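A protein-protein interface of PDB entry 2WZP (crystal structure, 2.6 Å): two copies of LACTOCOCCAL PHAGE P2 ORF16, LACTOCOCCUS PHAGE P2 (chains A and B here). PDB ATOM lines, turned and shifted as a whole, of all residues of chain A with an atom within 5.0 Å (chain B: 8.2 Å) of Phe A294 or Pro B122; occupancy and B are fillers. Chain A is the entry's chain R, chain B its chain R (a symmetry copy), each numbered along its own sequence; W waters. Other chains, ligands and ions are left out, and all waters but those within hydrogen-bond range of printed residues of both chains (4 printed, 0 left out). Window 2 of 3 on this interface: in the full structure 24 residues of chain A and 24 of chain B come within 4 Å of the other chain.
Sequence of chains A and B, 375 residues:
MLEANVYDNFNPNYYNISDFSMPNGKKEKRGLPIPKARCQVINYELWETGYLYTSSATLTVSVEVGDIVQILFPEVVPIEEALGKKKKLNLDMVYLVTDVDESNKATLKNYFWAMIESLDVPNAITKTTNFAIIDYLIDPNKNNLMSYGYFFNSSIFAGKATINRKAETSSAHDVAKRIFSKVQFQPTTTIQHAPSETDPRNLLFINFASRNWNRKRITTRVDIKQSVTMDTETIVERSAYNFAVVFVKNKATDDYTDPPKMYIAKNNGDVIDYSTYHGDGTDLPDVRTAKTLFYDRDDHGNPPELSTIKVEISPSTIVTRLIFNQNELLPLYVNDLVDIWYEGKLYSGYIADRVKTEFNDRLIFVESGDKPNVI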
ATOM      1  N   ILE A 163      16.458  -1.607  -8.004  1.00  0.00           N
ATOM      2  CA  ILE A 163      17.412  -2.641  -8.409  1.00  0.00           C
ATOM      3  C   ILE A 163      16.956  -4.079  -8.048  1.00  0.00           C
ATOM      4  O   ILE A 163      15.962  -4.256  -7.348  1.00  0.00           O
ATOM      5  CB  ILE A 163      18.823  -2.258  -7.891  1.00  0.00           C
ATOM      6  CG1 ILE A 163      18.900  -2.267  -6.343  1.00  0.00           C
ATOM      7  CG2 ILE A 163      19.263  -0.885  -8.463  1.00  0.00           C
ATOM      8  CD1 ILE A 163      20.253  -2.346  -5.845  1.00  0.00           C
ATOM      9  N   LYS A 166      20.181  -8.455  -4.265  1.00  0.00           N
ATOM     10  CA  LYS A 166      21.595  -8.850  -4.331  1.00  0.00           C
ATOM     11  C   LYS A 166      22.314  -8.364  -5.602  1.00  0.00           C
ATOM     12  O   LYS A 166      23.386  -8.853  -5.899  1.00  0.00           O
ATOM     13  CB  LYS A 166      21.776 -10.376  -4.047  1.00  0.00           C
ATOM     14  CG  LYS A 166      20.943 -10.863  -2.857  1.00  0.00           C
ATOM     15  CD  LYS A 166      21.365 -12.184  -2.251  1.00  0.00           C
ATOM     16  CE  LYS A 166      20.469 -13.326  -2.648  1.00  0.00           C
ATOM     17  NZ  LYS A 166      21.215 -14.616  -2.645  1.00  0.00           N
ATOM     18  N   ALA A 167      21.742  -7.367  -6.337  1.00  0.00           N
ATOM     19  CA  ALA A 167      22.286  -6.815  -7.599  1.00  0.00           C
ATOM     20  C   ALA A 167      22.564  -7.975  -8.595  1.00  0.00           C
ATOM     21  O   ALA A 167      23.580  -7.989  -9.296  1.00  0.00           O
ATOM     22  CB  ALA A 167      23.552  -5.997  -7.333  1.00  0.00           C
ATOM     23  N   PHE A 247      25.211  -1.141   0.513  1.00  0.00           N
ATOM     24  CA  PHE A 247      26.575  -1.579   0.194  1.00  0.00           C
ATOM     25  C   PHE A 247      26.984  -1.031  -1.163  1.00  0.00           C
ATOM     26  O   PHE A 247      26.202  -1.047  -2.123  1.00  0.00           O
ATOM     27  CB  PHE A 247      26.704  -3.102   0.173  1.00  0.00           C
ATOM     28  CG  PHE A 247      26.799  -3.722   1.546  1.00  0.00           C
ATOM     29  CD1 PHE A 247      28.028  -3.839   2.191  1.00  0.00           C
ATOM     30  CD2 PHE A 247      25.648  -4.166   2.212  1.00  0.00           C
ATOM     31  CE1 PHE A 247      28.106  -4.410   3.459  1.00  0.00           C
ATOM     32  CE2 PHE A 247      25.727  -4.727   3.480  1.00  0.00           C
ATOM     33  CZ  PHE A 247      26.955  -4.876   4.081  1.00  0.00           C
ATOM     34  N   TYR A 256      32.321  -5.876  -2.019  1.00  0.00           N
ATOM     35  CA  TYR A 256      31.637  -5.060  -1.017  1.00  0.00           C
ATOM     36  C   TYR A 256      32.390  -5.153   0.330  1.00  0.00           C
ATOM     37  O   TYR A 256      31.890  -5.736   1.294  1.00  0.00           O
ATOM     38  CB  TYR A 256      30.194  -5.540  -0.879  1.00  0.00           C
ATOM     39  CG  TYR A 256      29.447  -5.621  -2.186  1.00  0.00           C
ATOM     40  CD1 TYR A 256      28.887  -4.483  -2.765  1.00  0.00           C
ATOM     41  CD2 TYR A 256      29.241  -6.840  -2.816  1.00  0.00           C
ATOM     42  CE1 TYR A 256      28.205  -4.549  -3.984  1.00  0.00           C
ATOM     43  CE2 TYR A 256      28.560  -6.922  -4.034  1.00  0.00           C
ATOM     44  CZ  TYR A 256      28.029  -5.774  -4.610  1.00  0.00           C
ATOM     45  OH  TYR A 256      27.282  -5.873  -5.776  1.00  0.00           O
ATOM     46  N   THR A 292      18.416  -4.721   2.168  1.00  0.00           N
ATOM     47  CA  THR A 292      19.819  -4.553   1.846  1.00  0.00           C
ATOM     48  C   THR A 292      19.916  -4.276   0.401  1.00  0.00           C
ATOM     49  O   THR A 292      19.205  -4.911  -0.376  1.00  0.00           O
ATOM     50  CB  THR A 292      20.695  -5.685   2.387  1.00  0.00           C
ATOM     51  OG1 THR A 292      20.330  -5.922   3.734  1.00  0.00           O
ATOM     52  CG2 THR A 292      22.128  -5.334   2.378  1.00  0.00           C
ATOM     53  N   LEU A 293      20.747  -3.275   0.048  1.00  0.00           N
ATOM     54  CA  LEU A 293      20.998  -2.877  -1.318  1.00  0.00           C
ATOM     55  C   LEU A 293      22.468  -2.964  -1.687  1.00  0.00           C
ATOM     56  O   LEU A 293      23.344  -2.693  -0.865  1.00  0.00           O
ATOM     57  CB  LEU A 293      20.433  -1.484  -1.613  1.00  0.00           C
ATOM     58  CG  LEU A 293      18.932  -1.268  -1.333  1.00  0.00           C
ATOM     59  CD1 LEU A 293      18.603   0.213  -1.297  1.00  0.00           C
ATOM     60  CD2 LEU A 293      18.100  -1.929  -2.349  1.00  0.00           C
ATOM     61  N   PHE A 294      22.739  -3.338  -2.943  1.00  0.00           N
ATOM     62  CA  PHE A 294      24.099  -3.482  -3.454  1.00  0.00           C
ATOM     63  C   PHE A 294      24.264  -2.697  -4.743  1.00  0.00           C
ATOM     64  O   PHE A 294      23.472  -2.870  -5.666  1.00  0.00           O
ATOM     65  CB  PHE A 294      24.436  -4.969  -3.649  1.00  0.00           C
ATOM     66  CG  PHE A 294      24.379  -5.768  -2.371  1.00  0.00           C
ATOM     67  CD1 PHE A 294      25.506  -5.915  -1.574  1.00  0.00           C
ATOM     68  CD2 PHE A 294      23.184  -6.338  -1.939  1.00  0.00           C
ATOM     69  CE1 PHE A 294      25.446  -6.631  -0.377  1.00  0.00           C
ATOM     70  CE2 PHE A 294      23.127  -7.065  -0.757  1.00  0.00           C
ATOM     71  CZ  PHE A 294      24.259  -7.208   0.014  1.00  0.00           C
ATOM     72  N   TYR A 295      25.268  -1.814  -4.800  1.00  0.00           N
ATOM     73  CA  TYR A 295      25.556  -0.988  -5.978  1.00  0.00           C
ATOM     74  C   TYR A 295      27.029  -1.014  -6.322  1.00  0.00           C
ATOM     75  O   TYR A 295      27.872  -1.282  -5.464  1.00  0.00           O
ATOM     76  CB  TYR A 295      25.186   0.476  -5.727  1.00  0.00           C
ATOM     77  CG  TYR A 295      23.740   0.739  -5.375  1.00  0.00           C
ATOM     78  CD1 TYR A 295      22.821   1.109  -6.353  1.00  0.00           C
ATOM     79  CD2 TYR A 295      23.321   0.761  -4.048  1.00  0.00           C
ATOM     80  CE1 TYR A 295      21.505   1.425  -6.028  1.00  0.00           C
ATOM     81  CE2 TYR A 295      22.007   1.074  -3.713  1.00  0.00           C
ATOM     82  CZ  TYR A 295      21.100   1.399  -4.708  1.00  0.00           C
ATOM     83  OH  TYR A 295      19.805   1.701  -4.368  1.00  0.00           O
ATOM     84  N   ASP A 296      27.338  -0.693  -7.570  1.00  0.00           N
ATOM     85  CA  ASP A 296      28.698  -0.515  -8.042  1.00  0.00           C
ATOM     86  C   ASP A 296      28.905   1.006  -8.107  1.00  0.00           C
ATOM     87  O   ASP A 296      27.937   1.775  -8.045  1.00  0.00           O
ATOM     88  CB  ASP A 296      28.852  -1.084  -9.454  1.00  0.00           C
ATOM     89  CG  ASP A 296      29.078  -2.571  -9.577  1.00  0.00           C
ATOM     90  OD1 ASP A 296      28.929  -3.286  -8.558  1.00  0.00           O
ATOM     91  OD2 ASP A 296      29.367  -3.027 -10.698  1.00  0.00           O
ATOM     92  N   SER B 118      15.456  -9.811   6.543  1.00  0.00           N
ATOM     93  CA  SER B 118      15.759  -8.973   5.378  1.00  0.00           C
ATOM     94  C   SER B 118      17.155  -8.412   5.271  1.00  0.00           C
ATOM     95  O   SER B 118      17.444  -7.775   4.254  1.00  0.00           O
ATOM     96  CB  SER B 118      14.722  -7.874   5.197  1.00  0.00           C
ATOM     97  OG  SER B 118      13.393  -8.372   5.197  1.00  0.00           O
ATOM     98  N   LEU B 119      18.034  -8.655   6.281  1.00  0.00           N
ATOM     99  CA  LEU B 119      19.441  -8.229   6.249  1.00  0.00           C
ATOM    100  C   LEU B 119      20.238  -9.250   5.406  1.00  0.00           C
ATOM    101  O   LEU B 119      20.079 -10.460   5.594  1.00  0.00           O
ATOM    102  CB  LEU B 119      20.015  -8.156   7.690  1.00  0.00           C
ATOM    103  CG  LEU B 119      21.457  -7.640   7.827  1.00  0.00           C
ATOM    104  CD1 LEU B 119      21.565  -6.191   7.508  1.00  0.00           C
ATOM    105  CD2 LEU B 119      22.033  -7.963   9.182  1.00  0.00           C
ATOM    106  N   ASP B 120      21.084  -8.769   4.493  1.00  0.00           N
ATOM    107  CA  ASP B 120      21.903  -9.624   3.665  1.00  0.00           C
ATOM    108  C   ASP B 120      23.322  -9.448   4.029  1.00  0.00           C
ATOM    109  O   ASP B 120      23.746  -8.384   4.529  1.00  0.00           O
ATOM    110  CB  ASP B 120      21.699  -9.334   2.172  1.00  0.00           C
ATOM    111  CG  ASP B 120      20.318  -9.713   1.684  1.00  0.00           C
ATOM    112  OD1 ASP B 120      19.706 -10.649   2.281  1.00  0.00           O
ATOM    113  OD2 ASP B 120      19.848  -9.102   0.680  1.00  0.00           O
ATOM    114  N   VAL B 121      24.082 -10.515   3.789  1.00  0.00           N
ATOM    115  CA  VAL B 121      25.486 -10.530   4.079  1.00  0.00           C
ATOM    116  C   VAL B 121      26.334 -10.871   2.874  1.00  0.00           C
ATOM    117  O   VAL B 121      26.312 -11.998   2.405  1.00  0.00           O
ATOM    118  CB  VAL B 121      25.895 -11.125   5.470  1.00  0.00           C
ATOM    119  CG1 VAL B 121      24.794 -11.908   6.126  1.00  0.00           C
ATOM    120  CG2 VAL B 121      27.243 -11.844   5.509  1.00  0.00           C
ATOM    121  N   PRO B 122      27.057  -9.868   2.312  1.00  0.00           N
ATOM    122  CA  PRO B 122      27.967 -10.176   1.200  1.00  0.00           C
ATOM    123  C   PRO B 122      29.056 -11.132   1.691  1.00  0.00           C
ATOM    124  O   PRO B 122      29.319 -11.209   2.877  1.00  0.00           O
ATOM    125  CB  PRO B 122      28.511  -8.810   0.785  1.00  0.00           C
ATOM    126  CG  PRO B 122      28.325  -7.917   1.962  1.00  0.00           C
ATOM    127  CD  PRO B 122      27.159  -8.452   2.730  1.00  0.00           C
ATOM    128  N   ASN B 123      29.644 -11.911   0.799  1.00  0.00           N
ATOM    129  CA  ASN B 123      30.634 -12.877   1.197  1.00  0.00           C
ATOM    130  C   ASN B 123      31.808 -12.202   1.912  1.00  0.00           C
ATOM    131  O   ASN B 123      32.314 -12.749   2.888  1.00  0.00           O
ATOM    132  CB  ASN B 123      31.068 -13.701  -0.007  1.00  0.00           C
ATOM    133  CG  ASN B 123      31.722 -15.020   0.355  1.00  0.00           C
ATOM    134  OD1 ASN B 123      31.321 -15.732   1.277  1.00  0.00           O
ATOM    135  ND2 ASN B 123      32.753 -15.381  -0.360  1.00  0.00           N
ATOM    136  N   ALA B 124      32.187 -10.983   1.474  1.00  0.00           N
ATOM    137  CA  ALA B 124      33.278 -10.184   2.034  1.00  0.00           C
ATOM    138  C   ALA B 124      33.216 -10.009   3.556  1.00  0.00           C
ATOM    139  O   ALA B 124      34.249  -9.776   4.185  1.00  0.00           O
ATOM    140  CB  ALA B 124      33.332  -8.830   1.350  1.00  0.00           C
ATOM    141  N   ILE B 125      32.029 -10.141   4.155  1.00  0.00           N
ATOM    142  CA  ILE B 125      31.915 -10.030   5.605  1.00  0.00           C
ATOM    143  C   ILE B 125      32.464 -11.279   6.361  1.00  0.00           C
ATOM    144  O   ILE B 125      32.791 -11.184   7.547  1.00  0.00           O
ATOM    145  CB  ILE B 125      30.506  -9.570   6.021  1.00  0.00           C
ATOM    146  CG1 ILE B 125      30.250  -8.135   5.489  1.00  0.00           C
ATOM    147  CG2 ILE B 125      30.291  -9.676   7.558  1.00  0.00           C
ATOM    148  CD1 ILE B 125      28.900  -7.649   5.725  1.00  0.00           C
ATOM    149  N   THR B 126      32.634 -12.410   5.640  1.00  0.00           N
ATOM    150  CA  THR B 126      33.101 -13.708   6.151  1.00  0.00           C
ATOM    151  C   THR B 126      34.640 -13.830   6.145  1.00  0.00           C
ATOM    152  O   THR B 126      35.179 -14.873   6.505  1.00  0.00           O
ATOM    153  CB  THR B 126      32.452 -14.856   5.352  1.00  0.00           C
ATOM    154  OG1 THR B 126      33.066 -14.938   4.053  1.00  0.00           O
ATOM    155  CG2 THR B 126      30.927 -14.724   5.259  1.00  0.00           C
ATOM    156  N   LYS B 127      35.331 -12.769   5.698  1.00  0.00           N
ATOM    157  CA  LYS B 127      36.796 -12.748   5.549  1.00  0.00           C
ATOM    158  C   LYS B 127      37.666 -12.916   6.788  1.00  0.00           C
ATOM    159  O   LYS B 127      38.814 -13.340   6.704  1.00  0.00           O
ATOM    160  CB  LYS B 127      37.231 -11.532   4.735  1.00  0.00           C
ATOM    161  CG  LYS B 127      36.947 -11.636   3.265  1.00  0.00           C
ATOM    162  CD  LYS B 127      37.659 -10.508   2.566  1.00  0.00           C
ATOM    163  CE  LYS B 127      37.511 -10.617   1.081  1.00  0.00           C
ATOM    164  NZ  LYS B 127      38.260  -9.563   0.368  1.00  0.00           N
ATOM    165  N   ILE B 133      31.160 -11.338  12.054  1.00  0.00           N
ATOM    166  CA  ILE B 133      29.814 -11.567  11.530  1.00  0.00           C
ATOM    167  C   ILE B 133      28.777 -11.225  12.580  1.00  0.00           C
ATOM    168  O   ILE B 133      27.885 -10.452  12.287  1.00  0.00           O
ATOM    169  CB  ILE B 133      29.568 -12.936  10.848  1.00  0.00           C
ATOM    170  CG1 ILE B 133      30.570 -13.197   9.695  1.00  0.00           C
ATOM    171  CG2 ILE B 133      28.120 -12.990  10.308  1.00  0.00           C
ATOM    172  CD1 ILE B 133      30.751 -14.647   9.418  1.00  0.00           C
ATOM    173  N   TYR B 136      28.185  -7.622  13.039  1.00  0.00           N
ATOM    174  CA  TYR B 136      27.528  -7.052  11.859  1.00  0.00           C
ATOM    175  C   TYR B 136      26.010  -7.325  11.966  1.00  0.00           C
ATOM    176  O   TYR B 136      25.180  -6.428  11.774  1.00  0.00           O
ATOM    177  CB  TYR B 136      28.131  -7.616  10.556  1.00  0.00           C
ATOM    178  CG  TYR B 136      27.306  -7.293   9.325  1.00  0.00           C
ATOM    179  CD1 TYR B 136      27.268  -6.002   8.801  1.00  0.00           C
ATOM    180  CD2 TYR B 136      26.475  -8.251   8.747  1.00  0.00           C
ATOM    181  CE1 TYR B 136      26.458  -5.686   7.709  1.00  0.00           C
ATOM    182  CE2 TYR B 136      25.655  -7.941   7.663  1.00  0.00           C
ATOM    183  CZ  TYR B 136      25.664  -6.663   7.140  1.00  0.00           C
ATOM    184  OH  TYR B 136      24.856  -6.367   6.083  1.00  0.00           O
ATOM    185  N   ILE B 163      32.690 -19.498   4.845  1.00  0.00           N
ATOM    186  CA  ILE B 163      32.230 -18.690   3.713  1.00  0.00           C
ATOM    187  C   ILE B 163      30.745 -18.935   3.340  1.00  0.00           C
ATOM    188  O   ILE B 163      30.116 -19.847   3.870  1.00  0.00           O
ATOM    189  CB  ILE B 163      33.231 -18.850   2.539  1.00  0.00           C
ATOM    190  CG1 ILE B 163      33.250 -20.295   1.980  1.00  0.00           C
ATOM    191  CG2 ILE B 163      34.653 -18.397   2.965  1.00  0.00           C
ATOM    192  CD1 ILE B 163      33.816 -20.380   0.655  1.00  0.00           C
ATOM    193  N   ASN B 164      30.163 -18.096   2.492  1.00  0.00           N
ATOM    194  CA  ASN B 164      28.764 -18.309   2.093  1.00  0.00           C
ATOM    195  C   ASN B 164      28.708 -19.343   0.984  1.00  0.00           C
ATOM    196  O   ASN B 164      29.663 -19.397   0.209  1.00  0.00           O
ATOM    197  CB  ASN B 164      28.134 -16.999   1.604  1.00  0.00           C
ATOM    198  CG  ASN B 164      27.919 -15.974   2.674  1.00  0.00           C
ATOM    199  OD1 ASN B 164      27.850 -16.266   3.874  1.00  0.00           O
ATOM    200  ND2 ASN B 164      27.800 -14.744   2.257  1.00  0.00           N
ATOM    201  N   ALA B 167      30.096 -18.723  -2.675  1.00  0.00           N
ATOM    202  CA  ALA B 167      30.847 -17.462  -2.484  1.00  0.00           C
ATOM    203  C   ALA B 167      29.962 -16.261  -2.917  1.00  0.00           C
ATOM    204  O   ALA B 167      30.433 -15.312  -3.552  1.00  0.00           O
ATOM    205  CB  ALA B 167      32.165 -17.491  -3.264  1.00  0.00           C
ATOM    206  N   GLU B 168      28.676 -16.313  -2.577  1.00  0.00           N
ATOM    207  CA  GLU B 168      27.718 -15.298  -2.989  1.00  0.00           C
ATOM    208  C   GLU B 168      27.232 -14.507  -1.804  1.00  0.00           C
ATOM    209  O   GLU B 168      27.618 -14.801  -0.664  1.00  0.00           O
ATOM    210  CB  GLU B 168      26.495 -15.994  -3.613  1.00  0.00           C
ATOM    211  CG  GLU B 168      26.629 -16.493  -5.043  1.00  0.00           C
ATOM    212  CD  GLU B 168      25.402 -17.271  -5.521  1.00  0.00           C
ATOM    213  OE1 GLU B 168      24.476 -17.492  -4.697  1.00  0.00           O
ATOM    214  OE2 GLU B 168      25.372 -17.669  -6.717  1.00  0.00           O
ATOM    215  N   THR B 169      26.343 -13.523  -2.065  1.00  0.00           N
ATOM    216  CA  THR B 169      25.686 -12.775  -1.007  1.00  0.00           C
ATOM    217  C   THR B 169      24.590 -13.718  -0.459  1.00  0.00           C
ATOM    218  O   THR B 169      23.881 -14.339  -1.257  1.00  0.00           O
ATOM    219  CB  THR B 169      25.157 -11.459  -1.548  1.00  0.00           C
ATOM    220  OG1 THR B 169      26.298 -10.719  -1.967  1.00  0.00           O
ATOM    221  CG2 THR B 169      24.378 -10.671  -0.513  1.00  0.00           C
ATOM    222  N   SER B 170      24.525 -13.883   0.882  1.00  0.00           N
ATOM    223  CA  SER B 170      23.526 -14.752   1.520  1.00  0.00           C
ATOM    224  C   SER B 170      22.711 -13.907   2.479  1.00  0.00           C
ATOM    225  O   SER B 170      23.116 -12.794   2.809  1.00  0.00           O
ATOM    226  CB  SER B 170      24.191 -15.902   2.288  1.00  0.00           C
ATOM    227  OG  SER B 170      24.733 -16.890   1.426  1.00  0.00           O
ATOM    228  N   SER B 171      21.570 -14.431   2.935  1.00  0.00           N
ATOM    229  CA  SER B 171      20.745 -13.733   3.913  1.00  0.00           C
ATOM    230  C   SER B 171      21.362 -13.913   5.290  1.00  0.00           C
ATOM    231  O   SER B 171      21.927 -14.958   5.537  1.00  0.00           O
ATOM    232  CB  SER B 171      19.327 -14.301   3.905  1.00  0.00           C
ATOM    233  OG  SER B 171      19.230 -15.606   4.446  1.00  0.00           O
ATOM    234  N   ALA B 172      21.190 -12.941   6.200  1.00  0.00           N
ATOM    235  CA  ALA B 172      21.649 -12.999   7.598  1.00  0.00           C
ATOM    236  C   ALA B 172      21.052 -14.242   8.277  1.00  0.00           C
ATOM    237  O   ALA B 172      21.735 -14.897   9.042  1.00  0.00           O
ATOM    238  CB  ALA B 172      21.231 -11.740   8.333  1.00  0.00           C
ATOM    239  N   VAL B 175      23.345 -17.115   7.146  1.00  0.00           N
ATOM    240  CA  VAL B 175      24.683 -17.089   7.718  1.00  0.00           C
ATOM    241  C   VAL B 175      24.740 -17.344   9.230  1.00  0.00           C
ATOM    242  O   VAL B 175      25.641 -18.047   9.702  1.00  0.00           O
ATOM    243  CB  VAL B 175      25.675 -16.036   7.157  1.00  0.00           C
ATOM    244  CG1 VAL B 175      25.042 -15.160   6.111  1.00  0.00           C
ATOM    245  CG2 VAL B 175      26.371 -15.246   8.241  1.00  0.00           C
ATOM    246  N   ARG B 178      24.352 -21.015   9.817  1.00  0.00           N
ATOM    247  CA  ARG B 178      25.649 -21.624   9.520  1.00  0.00           C
ATOM    248  C   ARG B 178      26.607 -21.489  10.672  1.00  0.00           C
ATOM    249  O   ARG B 178      27.165 -22.485  11.095  1.00  0.00           O
ATOM    250  CB  ARG B 178      26.272 -21.091   8.218  1.00  0.00           C
ATOM    251  CG  ARG B 178      27.654 -21.694   7.969  1.00  0.00           C
ATOM    252  CD  ARG B 178      28.249 -21.308   6.666  1.00  0.00           C
ATOM    253  NE  ARG B 178      28.787 -19.947   6.690  1.00  0.00           N
ATOM    254  CZ  ARG B 178      28.233 -18.907   6.079  1.00  0.00           C
ATOM    255  NH1 ARG B 178      27.103 -19.054   5.397  1.00  0.00           N
ATOM    256  NH2 ARG B 178      28.837 -17.736   6.082  1.00  0.00           N
HETATM  257  O   HOH W   1      19.772  -7.278  -1.650  1.00  0.00           O
HETATM  258  O   HOH W   2      17.991  -5.245   5.395  1.00  0.00           O
HETATM  259  O   HOH W   3      25.239  -9.509  -4.180  1.00  0.00           O
HETATM  260  O   HOH W   4      16.985  -7.321   1.760  1.00  0.00           O
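Positions printed for both chains: 163 and 167.
Hydrophobic or aromatic side chains of chain B that line the printed part of chain A: Leu B119, Pro B122, Ala B124, Ile B125 and Tyr B136.
Of the 10 printed residues of chain A, 5 touch a printed residue of chain B.
Among the printed residues, no Asp or Glu carboxylate lies within 4 Å of a Lys or Arg side-chain nitrogen of the other chain.
NZ of Lys A166 sits at hydrogen-bond distance from O of Thr B169, at 3.0 Å.
The side-chain hydroxyl (OG1) of Thr A292 is in hydrogen-bond range of the backbone carbonyl oxygen (O) of Ser B118, at 3.5 Å.
OG1 of Thr A292 is in hydrogen-bond range of N of Asp B120, at 3.0 Å.
N of Phe A247 lies within hydrogen-bond range of O of Leu A293, 2.8 Å away.
The backbone NH of Tyr A295 is in hydrogen-bond range of the backbone carbonyl oxygen of Phe A247, 2.9 Å away.
The backbone NH of Ala B172 sits at hydrogen-bond distance from the backbone carbonyl oxygen of Leu B119.
O of Asp B120 is in hydrogen-bond range of OH of Tyr B136.
Among the printed residues, pairs that only touch across the chains: Phe A247 with Pro B122 (3.8 Å), Phe A247 with Ile B125 (3.8 Å), Phe A247 with Tyr B136 (3.2 Å), Tyr A256 with Ala B124 (3.4 Å), Thr A292 with Leu B119 (3.5 Å), Phe A294 with Asp B120 (3.97 Å), Phe A294 with Pro B122 (3.9 Å) and Phe A294 with Thr B169 (3.5 Å).
Of the printed residues of chain B, Phe A247 touches Pro B122 (3.8 Å), Ile B125 (3.8 Å) and Tyr B136 (3.2 Å).
Of chain B, only Asp B120, Pro B122 and Thr B169 come within 4 Å of Phe A294.
Printed residues of chain A within 4 Å of Ser B118: Thr A292 (3.5 Å).
Pro B122 touches just these residues of chain A: Phe A247 and Phe A294.
Of the printed residues of chain A, Ala B124 touches Tyr A256 (3.4 Å).
Printed residues of chain A within 4 Å of Tyr B136: Phe A247 (3.2 Å).
Asn B164 touches none of the printed residues of chain A.
Glu B168 touches none of the printed residues of chain A.
The nearest residue of chain A that does not touch Pro B122 is Tyr A256 (4.04 Å).
The nearest printed residue of chain A that does not touch Leu B119 is Phe A247 (6.0 Å).
Water W4 bridges O of Ser B118 (2.6 Å) and N of Thr A292 (3.0 Å).
Water W3 lies within hydrogen-bond range of the backbone carbonyl oxygen (O) of Lys A166 (2.6 Å) and the side-chain hydroxyl (OG1) of Thr B169 (2.7 Å).
Water W1 lies within hydrogen-bond range of the backbone carbonyl oxygen of Thr A292 (2.7 Å), the backbone NH of Lys A166 (2.9 Å) and the side-chain carboxylate of Asp B120 (3.0 Å).
Water W2 lies within hydrogen-bond range of the backbone carbonyl oxygen of Ser B118 and the side-chain hydroxyl of Thr A292.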
